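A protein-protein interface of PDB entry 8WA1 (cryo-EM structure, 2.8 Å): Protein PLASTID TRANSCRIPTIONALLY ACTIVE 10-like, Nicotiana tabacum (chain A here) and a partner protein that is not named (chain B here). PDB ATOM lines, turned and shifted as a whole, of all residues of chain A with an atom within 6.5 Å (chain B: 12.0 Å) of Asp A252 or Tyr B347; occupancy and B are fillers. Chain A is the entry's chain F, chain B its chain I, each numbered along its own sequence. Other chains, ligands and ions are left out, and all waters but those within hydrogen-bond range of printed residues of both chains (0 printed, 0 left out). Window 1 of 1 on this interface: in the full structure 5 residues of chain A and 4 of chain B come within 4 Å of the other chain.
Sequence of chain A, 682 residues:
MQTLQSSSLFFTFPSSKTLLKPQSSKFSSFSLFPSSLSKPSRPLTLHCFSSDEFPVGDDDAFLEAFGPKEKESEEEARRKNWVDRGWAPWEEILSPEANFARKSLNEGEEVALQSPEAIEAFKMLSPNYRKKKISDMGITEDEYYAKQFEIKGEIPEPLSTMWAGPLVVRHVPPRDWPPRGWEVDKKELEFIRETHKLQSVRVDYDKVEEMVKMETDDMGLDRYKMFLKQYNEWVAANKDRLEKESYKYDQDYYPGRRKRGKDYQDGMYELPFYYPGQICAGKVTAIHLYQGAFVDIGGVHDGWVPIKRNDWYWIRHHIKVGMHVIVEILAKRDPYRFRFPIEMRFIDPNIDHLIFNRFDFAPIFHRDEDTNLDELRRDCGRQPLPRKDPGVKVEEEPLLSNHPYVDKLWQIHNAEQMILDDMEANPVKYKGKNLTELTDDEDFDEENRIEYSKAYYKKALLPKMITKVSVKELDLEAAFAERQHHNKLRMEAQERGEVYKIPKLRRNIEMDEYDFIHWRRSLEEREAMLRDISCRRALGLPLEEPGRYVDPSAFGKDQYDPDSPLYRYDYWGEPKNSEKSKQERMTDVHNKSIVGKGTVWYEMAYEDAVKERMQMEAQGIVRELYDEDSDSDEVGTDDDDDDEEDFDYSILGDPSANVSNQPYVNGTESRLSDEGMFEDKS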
ATOM      1  N   ASP A 250      27.588 -31.909 -18.963  1.00  0.00           N
ATOM      2  CA  ASP A 250      27.263 -30.833 -19.893  1.00  0.00           C
ATOM      3  C   ASP A 250      27.805 -31.178 -21.272  1.00  0.00           C
ATOM      4  O   ASP A 250      28.979 -31.540 -21.408  1.00  0.00           O
ATOM      5  CB  ASP A 250      27.831 -29.498 -19.405  1.00  0.00           C
ATOM      6  CG  ASP A 250      27.217 -29.048 -18.094  1.00  0.00           C
ATOM      7  OD1 ASP A 250      26.051 -29.409 -17.827  1.00  0.00           O
ATOM      8  OD2 ASP A 250      27.898 -28.332 -17.331  1.00  0.00           O
ATOM      9  N   GLN A 251      26.949 -31.070 -22.291  1.00  0.00           N
ATOM     10  CA  GLN A 251      27.365 -31.411 -23.648  1.00  0.00           C
ATOM     11  C   GLN A 251      28.024 -30.235 -24.358  1.00  0.00           C
ATOM     12  O   GLN A 251      29.038 -30.415 -25.039  1.00  0.00           O
ATOM     13  CB  GLN A 251      26.170 -31.905 -24.462  1.00  0.00           C
ATOM     14  CG  GLN A 251      25.635 -33.262 -24.040  1.00  0.00           C
ATOM     15  CD  GLN A 251      24.533 -33.758 -24.955  1.00  0.00           C
ATOM     16  OE1 GLN A 251      24.145 -33.076 -25.904  1.00  0.00           O
ATOM     17  NE2 GLN A 251      24.022 -34.952 -24.674  1.00  0.00           N
ATOM     18  N   ASP A 252      27.471 -29.032 -24.212  1.00  0.00           N
ATOM     19  CA  ASP A 252      27.951 -27.868 -24.943  1.00  0.00           C
ATOM     20  C   ASP A 252      28.251 -26.740 -23.968  1.00  0.00           C
ATOM     21  O   ASP A 252      27.637 -26.638 -22.903  1.00  0.00           O
ATOM     22  CB  ASP A 252      26.928 -27.393 -25.984  1.00  0.00           C
ATOM     23  CG  ASP A 252      26.619 -28.451 -27.023  1.00  0.00           C
ATOM     24  OD1 ASP A 252      27.520 -29.256 -27.337  1.00  0.00           O
ATOM     25  OD2 ASP A 252      25.477 -28.477 -27.526  1.00  0.00           O
ATOM     26  N   TYR A 253      29.205 -25.894 -24.346  1.00  0.00           N
ATOM     27  CA  TYR A 253      29.560 -24.754 -23.514  1.00  0.00           C
ATOM     28  C   TYR A 253      28.549 -23.629 -23.689  1.00  0.00           C
ATOM     29  O   TYR A 253      28.062 -23.373 -24.793  1.00  0.00           O
ATOM     30  CB  TYR A 253      30.963 -24.254 -23.856  1.00  0.00           C
ATOM     31  CG  TYR A 253      31.324 -22.962 -23.160  1.00  0.00           C
ATOM     32  CD1 TYR A 253      31.661 -22.948 -21.815  1.00  0.00           C
ATOM     33  CD2 TYR A 253      31.326 -21.755 -23.850  1.00  0.00           C
ATOM     34  CE1 TYR A 253      31.989 -21.771 -21.173  1.00  0.00           C
ATOM     35  CE2 TYR A 253      31.654 -20.572 -23.215  1.00  0.00           C
ATOM     36  CZ  TYR A 253      31.985 -20.586 -21.877  1.00  0.00           C
ATOM     37  OH  TYR A 253      32.312 -19.412 -21.239  1.00  0.00           O
ATOM     38  N   TYR A 254      28.238 -22.955 -22.589  1.00  0.00           N
ATOM     39  CA  TYR A 254      27.304 -21.842 -22.585  1.00  0.00           C
ATOM     40  C   TYR A 254      27.773 -20.838 -21.546  1.00  0.00           C
ATOM     41  O   TYR A 254      28.376 -21.224 -20.538  1.00  0.00           O
ATOM     42  CB  TYR A 254      25.875 -22.317 -22.281  1.00  0.00           C
ATOM     43  CG  TYR A 254      24.814 -21.263 -22.485  1.00  0.00           C
ATOM     44  CD1 TYR A 254      24.275 -21.029 -23.743  1.00  0.00           C
ATOM     45  CD2 TYR A 254      24.350 -20.502 -21.421  1.00  0.00           C
ATOM     46  CE1 TYR A 254      23.305 -20.066 -23.935  1.00  0.00           C
ATOM     47  CE2 TYR A 254      23.380 -19.536 -21.604  1.00  0.00           C
ATOM     48  CZ  TYR A 254      22.861 -19.322 -22.862  1.00  0.00           C
ATOM     49  OH  TYR A 254      21.894 -18.363 -23.052  1.00  0.00           O
ATOM     50  N   ARG A 257      28.970 -21.669 -17.753  1.00  0.00           N
ATOM     51  CA  ARG A 257      29.410 -23.048 -17.627  1.00  0.00           C
ATOM     52  C   ARG A 257      30.929 -23.080 -17.521  1.00  0.00           C
ATOM     53  O   ARG A 257      31.615 -22.090 -17.784  1.00  0.00           O
ATOM     54  CB  ARG A 257      28.946 -23.903 -18.815  1.00  0.00           C
ATOM     55  CG  ARG A 257      27.437 -24.076 -18.937  1.00  0.00           C
ATOM     56  CD  ARG A 257      26.890 -25.045 -17.897  1.00  0.00           C
ATOM     57  NE  ARG A 257      26.669 -24.406 -16.604  1.00  0.00           N
ATOM     58  CZ  ARG A 257      26.299 -25.054 -15.504  1.00  0.00           C
ATOM     59  NH1 ARG A 257      26.110 -26.366 -15.539  1.00  0.00           N
ATOM     60  NH2 ARG A 257      26.119 -24.391 -14.371  1.00  0.00           N
ATOM     61  N   ARG A 260      36.319 -25.418 -20.785  1.00  0.00           N
ATOM     62  CA  ARG A 260      37.044 -26.669 -20.944  1.00  0.00           C
ATOM     63  C   ARG A 260      37.705 -26.713 -22.314  1.00  0.00           C
ATOM     64  O   ARG A 260      37.449 -25.876 -23.183  1.00  0.00           O
ATOM     65  CB  ARG A 260      36.107 -27.871 -20.766  1.00  0.00           C
ATOM     66  CG  ARG A 260      34.952 -27.889 -21.755  1.00  0.00           C
ATOM     67  CD  ARG A 260      33.815 -28.768 -21.269  1.00  0.00           C
ATOM     68  NE  ARG A 260      32.692 -28.762 -22.200  1.00  0.00           N
ATOM     69  CZ  ARG A 260      31.500 -29.283 -21.936  1.00  0.00           C
ATOM     70  NH1 ARG A 260      31.268 -29.850 -20.760  1.00  0.00           N
ATOM     71  NH2 ARG A 260      30.536 -29.231 -22.845  1.00  0.00           N
ATOM     72  N   GLN A 291      18.089 -13.595 -20.721  1.00  0.00           N
ATOM     73  CA  GLN A 291      18.786 -13.980 -19.498  1.00  0.00           C
ATOM     74  C   GLN A 291      19.524 -12.800 -18.877  1.00  0.00           C
ATOM     75  O   GLN A 291      19.409 -12.556 -17.670  1.00  0.00           O
ATOM     76  CB  GLN A 291      19.748 -15.129 -19.791  1.00  0.00           C
ATOM     77  CG  GLN A 291      19.081 -16.316 -20.462  1.00  0.00           C
ATOM     78  CD  GLN A 291      20.038 -17.461 -20.715  1.00  0.00           C
ATOM     79  OE1 GLN A 291      21.246 -17.327 -20.523  1.00  0.00           O
ATOM     80  NE2 GLN A 291      19.502 -18.595 -21.146  1.00  0.00           N
ATOM     81  N   ARG A 339      22.011 -22.854 -13.565  1.00  0.00           N
ATOM     82  CA  ARG A 339      22.632 -22.530 -14.845  1.00  0.00           C
ATOM     83  C   ARG A 339      23.739 -21.499 -14.679  1.00  0.00           C
ATOM     84  O   ARG A 339      24.762 -21.560 -15.371  1.00  0.00           O
ATOM     85  CB  ARG A 339      21.576 -22.028 -15.829  1.00  0.00           C
ATOM     86  CG  ARG A 339      20.503 -23.049 -16.168  1.00  0.00           C
ATOM     87  CD  ARG A 339      19.571 -22.522 -17.245  1.00  0.00           C
ATOM     88  NE  ARG A 339      20.281 -22.244 -18.490  1.00  0.00           N
ATOM     89  CZ  ARG A 339      19.716 -21.721 -19.572  1.00  0.00           C
ATOM     90  NH1 ARG A 339      18.426 -21.414 -19.564  1.00  0.00           N
ATOM     91  NH2 ARG A 339      20.438 -21.503 -20.661  1.00  0.00           N
ATOM     92  N   PHE A 365      18.637 -26.196 -13.537  1.00  0.00           N
ATOM     93  CA  PHE A 365      18.689 -27.227 -14.566  1.00  0.00           C
ATOM     94  C   PHE A 365      17.687 -28.324 -14.230  1.00  0.00           C
ATOM     95  O   PHE A 365      17.728 -28.895 -13.135  1.00  0.00           O
ATOM     96  CB  PHE A 365      20.093 -27.817 -14.684  1.00  0.00           C
ATOM     97  CG  PHE A 365      20.986 -27.083 -15.642  1.00  0.00           C
ATOM     98  CD1 PHE A 365      20.700 -27.059 -16.996  1.00  0.00           C
ATOM     99  CD2 PHE A 365      22.124 -26.438 -15.191  1.00  0.00           C
ATOM    100  CE1 PHE A 365      21.525 -26.391 -17.881  1.00  0.00           C
ATOM    101  CE2 PHE A 365      22.953 -25.771 -16.071  1.00  0.00           C
ATOM    102  CZ  PHE A 365      22.652 -25.746 -17.417  1.00  0.00           C
ATOM    103  N   ARG B 339      26.010 -42.619 -32.959  1.00  0.00           N
ATOM    104  CA  ARG B 339      25.963 -41.551 -31.964  1.00  0.00           C
ATOM    105  C   ARG B 339      26.049 -40.180 -32.624  1.00  0.00           C
ATOM    106  O   ARG B 339      25.469 -39.208 -32.127  1.00  0.00           O
ATOM    107  CB  ARG B 339      27.092 -41.731 -30.949  1.00  0.00           C
ATOM    108  CG  ARG B 339      26.832 -42.810 -29.913  1.00  0.00           C
ATOM    109  CD  ARG B 339      28.088 -43.616 -29.631  1.00  0.00           C
ATOM    110  NE  ARG B 339      29.245 -42.764 -29.371  1.00  0.00           N
ATOM    111  CZ  ARG B 339      30.488 -43.215 -29.246  1.00  0.00           C
ATOM    112  NH1 ARG B 339      30.740 -44.512 -29.358  1.00  0.00           N
ATOM    113  NH2 ARG B 339      31.483 -42.370 -29.011  1.00  0.00           N
ATOM    114  N   LYS B 340      26.772 -40.083 -33.742  1.00  0.00           N
ATOM    115  CA  LYS B 340      26.892 -38.807 -34.442  1.00  0.00           C
ATOM    116  C   LYS B 340      25.555 -38.358 -35.018  1.00  0.00           C
ATOM    117  O   LYS B 340      25.167 -37.193 -34.868  1.00  0.00           O
ATOM    118  CB  LYS B 340      27.938 -38.907 -35.550  1.00  0.00           C
ATOM    119  CG  LYS B 340      29.375 -38.858 -35.068  1.00  0.00           C
ATOM    120  CD  LYS B 340      30.340 -38.956 -36.239  1.00  0.00           C
ATOM    121  CE  LYS B 340      30.087 -37.862 -37.261  1.00  0.00           C
ATOM    122  NZ  LYS B 340      30.248 -36.505 -36.670  1.00  0.00           N
ATOM    123  N   ASN B 342      22.658 -39.010 -34.076  1.00  0.00           N
ATOM    124  CA  ASN B 342      21.714 -38.716 -33.006  1.00  0.00           C
ATOM    125  C   ASN B 342      22.080 -37.472 -32.207  1.00  0.00           C
ATOM    126  O   ASN B 342      21.385 -37.152 -31.237  1.00  0.00           O
ATOM    127  CB  ASN B 342      21.598 -39.914 -32.060  1.00  0.00           C
ATOM    128  CG  ASN B 342      20.976 -41.125 -32.726  1.00  0.00           C
ATOM    129  OD1 ASN B 342      20.207 -40.996 -33.678  1.00  0.00           O
ATOM    130  ND2 ASN B 342      21.304 -42.309 -32.224  1.00  0.00           N
ATOM    131  N   TYR B 343      23.146 -36.768 -32.581  1.00  0.00           N
ATOM    132  CA  TYR B 343      23.542 -35.572 -31.851  1.00  0.00           C
ATOM    133  C   TYR B 343      22.577 -34.428 -32.134  1.00  0.00           C
ATOM    134  O   TYR B 343      22.221 -34.171 -33.288  1.00  0.00           O
ATOM    135  CB  TYR B 343      24.967 -35.166 -32.229  1.00  0.00           C
ATOM    136  CG  TYR B 343      25.404 -33.852 -31.620  1.00  0.00           C
ATOM    137  CD1 TYR B 343      25.799 -33.778 -30.292  1.00  0.00           C
ATOM    138  CD2 TYR B 343      25.423 -32.686 -32.375  1.00  0.00           C
ATOM    139  CE1 TYR B 343      26.196 -32.581 -29.730  1.00  0.00           C
ATOM    140  CE2 TYR B 343      25.819 -31.484 -31.822  1.00  0.00           C
ATOM    141  CZ  TYR B 343      26.205 -31.437 -30.500  1.00  0.00           C
ATOM    142  OH  TYR B 343      26.601 -30.242 -29.945  1.00  0.00           O
ATOM    143  N   ARG B 344      22.157 -33.740 -31.074  1.00  0.00           N
ATOM    144  CA  ARG B 344      21.254 -32.598 -31.182  1.00  0.00           C
ATOM    145  C   ARG B 344      21.865 -31.434 -30.413  1.00  0.00           C
ATOM    146  O   ARG B 344      22.372 -31.636 -29.290  1.00  0.00           O
ATOM    147  CB  ARG B 344      19.861 -32.935 -30.646  1.00  0.00           C
ATOM    148  CG  ARG B 344      18.809 -33.161 -31.722  1.00  0.00           C
ATOM    149  CD  ARG B 344      19.085 -34.416 -32.532  1.00  0.00           C
ATOM    150  NE  ARG B 344      18.057 -34.644 -33.543  1.00  0.00           N
ATOM    151  CZ  ARG B 344      18.048 -35.676 -34.381  1.00  0.00           C
ATOM    152  NH1 ARG B 344      19.015 -36.581 -34.331  1.00  0.00           N
ATOM    153  NH2 ARG B 344      17.071 -35.804 -35.269  1.00  0.00           N
ATOM    154  N   PRO B 345      21.857 -30.219 -30.961  1.00  0.00           N
ATOM    155  CA  PRO B 345      22.383 -29.073 -30.208  1.00  0.00           C
ATOM    156  C   PRO B 345      21.493 -28.760 -29.013  1.00  0.00           C
ATOM    157  O   PRO B 345      20.266 -28.730 -29.128  1.00  0.00           O
ATOM    158  CB  PRO B 345      22.377 -27.935 -31.235  1.00  0.00           C
ATOM    159  N   GLN B 346      22.123 -28.532 -27.860  1.00  0.00           N
ATOM    160  CA  GLN B 346      21.361 -28.336 -26.630  1.00  0.00           C
ATOM    161  C   GLN B 346      20.742 -26.944 -26.573  1.00  0.00           C
ATOM    162  O   GLN B 346      19.537 -26.800 -26.338  1.00  0.00           O
ATOM    163  CB  GLN B 346      22.257 -28.577 -25.415  1.00  0.00           C
ATOM    164  CG  GLN B 346      21.541 -28.427 -24.084  1.00  0.00           C
ATOM    165  CD  GLN B 346      22.452 -28.676 -22.900  1.00  0.00           C
ATOM    166  OE1 GLN B 346      22.025 -28.609 -21.748  1.00  0.00           O
ATOM    167  NE2 GLN B 346      23.717 -28.967 -23.178  1.00  0.00           N
ATOM    168  N   TYR B 347      21.550 -25.906 -26.784  1.00  0.00           N
ATOM    169  CA  TYR B 347      21.095 -24.528 -26.631  1.00  0.00           C
ATOM    170  C   TYR B 347      20.717 -23.878 -27.957  1.00  0.00           C
ATOM    171  O   TYR B 347      19.591 -23.396 -28.111  1.00  0.00           O
ATOM    172  CB  TYR B 347      22.175 -23.694 -25.930  1.00  0.00           C
ATOM    173  CG  TYR B 347      22.538 -24.207 -24.556  1.00  0.00           C
ATOM    174  CD1 TYR B 347      21.783 -23.862 -23.444  1.00  0.00           C
ATOM    175  CD2 TYR B 347      23.635 -25.036 -24.372  1.00  0.00           C
ATOM    176  CE1 TYR B 347      22.110 -24.329 -22.186  1.00  0.00           C
ATOM    177  CE2 TYR B 347      23.970 -25.508 -23.117  1.00  0.00           C
ATOM    178  CZ  TYR B 347      23.204 -25.152 -22.029  1.00  0.00           C
ATOM    179  OH  TYR B 347      23.532 -25.617 -20.777  1.00  0.00           O
ATOM    180  N   PHE B 348      21.633 -23.855 -28.922  1.00  0.00           N
ATOM    181  CA  PHE B 348      21.362 -23.237 -30.212  1.00  0.00           C
ATOM    182  C   PHE B 348      22.134 -23.974 -31.295  1.00  0.00           C
ATOM    183  O   PHE B 348      23.185 -24.567 -31.037  1.00  0.00           O
ATOM    184  CB  PHE B 348      21.727 -21.748 -30.210  1.00  0.00           C
ATOM    185  CG  PHE B 348      22.970 -21.429 -29.429  1.00  0.00           C
ATOM    186  CD1 PHE B 348      24.223 -21.650 -29.972  1.00  0.00           C
ATOM    187  CD2 PHE B 348      22.881 -20.911 -28.148  1.00  0.00           C
ATOM    188  CE1 PHE B 348      25.367 -21.359 -29.253  1.00  0.00           C
ATOM    189  CE2 PHE B 348      24.021 -20.616 -27.424  1.00  0.00           C
ATOM    190  CZ  PHE B 348      25.265 -20.841 -27.977  1.00  0.00           C
ATOM    191  N   ALA B 349      21.600 -23.929 -32.512  1.00  0.00           N
ATOM    192  CA  ALA B 349      22.225 -24.590 -33.643  1.00  0.00           C
ATOM    193  C   ALA B 349      23.359 -23.736 -34.207  1.00  0.00           C
ATOM    194  O   ALA B 349      23.502 -22.552 -33.892  1.00  0.00           O
ATOM    195  CB  ALA B 349      21.191 -24.885 -34.728  1.00  0.00           C
ATOM    196  N   GLU B 350      24.175 -24.360 -35.057  1.00  0.00           N
ATOM    197  CA  GLU B 350      25.300 -23.687 -35.695  1.00  0.00           C
ATOM    198  C   GLU B 350      25.159 -23.624 -37.211  1.00  0.00           C
ATOM    199  O   GLU B 350      26.092 -23.184 -37.892  1.00  0.00           O
ATOM    200  CB  GLU B 350      26.615 -24.378 -35.322  1.00  0.00           C
ATOM    201  N   ASN B 351      24.021 -24.050 -37.755  1.00  0.00           N
ATOM    202  CA  ASN B 351      23.818 -24.053 -39.196  1.00  0.00           C
ATOM    203  C   ASN B 351      22.322 -24.084 -39.478  1.00  0.00           C
ATOM    204  O   ASN B 351      21.501 -24.264 -38.576  1.00  0.00           O
ATOM    205  CB  ASN B 351      24.527 -25.240 -39.856  1.00  0.00           C
ATOM    206  N   GLN B 354      20.531 -27.783 -39.099  1.00  0.00           N
ATOM    207  CA  GLN B 354      20.128 -28.216 -37.765  1.00  0.00           C
ATOM    208  C   GLN B 354      18.828 -27.550 -37.333  1.00  0.00           C
ATOM    209  O   GLN B 354      18.075 -28.107 -36.526  1.00  0.00           O
ATOM    210  CB  GLN B 354      21.243 -27.923 -36.762  1.00  0.00           C
ATOM    211  CG  GLN B 354      22.566 -28.576 -37.109  1.00  0.00           C
ATOM    212  CD  GLN B 354      23.649 -28.264 -36.097  1.00  0.00           C
ATOM    213  OE1 GLN B 354      23.394 -27.623 -35.079  1.00  0.00           O
ATOM    214  NE2 GLN B 354      24.865 -28.716 -36.374  1.00  0.00           N
ATOM    215  N   THR B 355      18.547 -26.355 -37.855  1.00  0.00           N
ATOM    216  CA  THR B 355      17.341 -25.639 -37.455  1.00  0.00           C
ATOM    217  C   THR B 355      16.087 -26.311 -38.003  1.00  0.00           C
ATOM    218  O   THR B 355      15.061 -26.383 -37.316  1.00  0.00           O
ATOM    219  CB  THR B 355      17.412 -24.185 -37.918  1.00  0.00           C
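The side-chain carboxylate of Asp A252 is in hydrogen-bond range of the side-chain hydroxyl of Tyr B343 (2.9 Å).
OD2 of Asp A252 sits at hydrogen-bond distance from N of Gln B346 (3.4 Å).
The backbone carbonyl oxygen of Gln A251 lies within hydrogen-bond range of the guanidinium group of Arg A260.
The side-chain amide oxygen of Gln A291 is in hydrogen-bond range of the side-chain hydroxyl of Tyr A254 (2.8 Å).
The backbone carbonyl oxygen of Arg A339 sits at hydrogen-bond distance from the guanidinium group of Arg A257 (3.3 Å).
The side-chain amide nitrogen of Gln A291 lies close to the guanidinium group of Arg A339 (3.1 Å).
OE1 of Gln B346 lies within hydrogen-bond range of OH of Tyr B347 (3.5 Å).
N of Gln A251 touches NE2 of Gln B346, 3.96 Å away.
Tyr B347 touches Asp A252.
Tyr A254 touches Tyr B347.
Phe B348 touches Tyr A254 (CE2 to CE1, 3.6 Å).
Arg A339 touches Tyr B347.
Phe A365 touches Tyr B347 (CZ to OH, 3.5 Å).
Of chain B, only Gln B346 (3.96 Å) comes within 4 Å of Gln A251.
Asp A252 touches just these residues of chain B: Tyr B343 (2.9 Å), Gln B346 (3.4 Å) and Tyr B347 (3.8 Å).
Tyr A253 touches none of the printed residues of chain B.
No residue of chain B comes within 4 Å of Arg A257.
Of chain B, only Tyr B347 (3.6 Å) comes within 4 Å of Arg A339.
Printed residues of chain A within 4 Å of Gln B346: Gln A251 and Asp A252.
Printed residues of chain A within 4 Å of Phe B348: Tyr A254 (3.6 Å).
The nearest printed residue of chain A that does not touch Tyr B343 is Gln A251 (4.4 Å).
Of the 10 printed residues of chain A, 5 touch a printed residue of chain B.
Printed residues of chain A that touch a printed residue of chain B: Gln A251, Asp A252, Tyr A254, Arg A339 and Phe A365.
Hydrophobic or aromatic side chains of chain A that line the printed part of chain B: Tyr A254 and Phe A365.
Hydrophobic or aromatic side chains of chain B within 4 Å of the printed part of chain A: Tyr B343, Tyr B347 and Phe B348.
Among the printed residues, no Asp or Glu carboxylate lies within 4 Å of a Lys or Arg side-chain nitrogen of the other chain.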
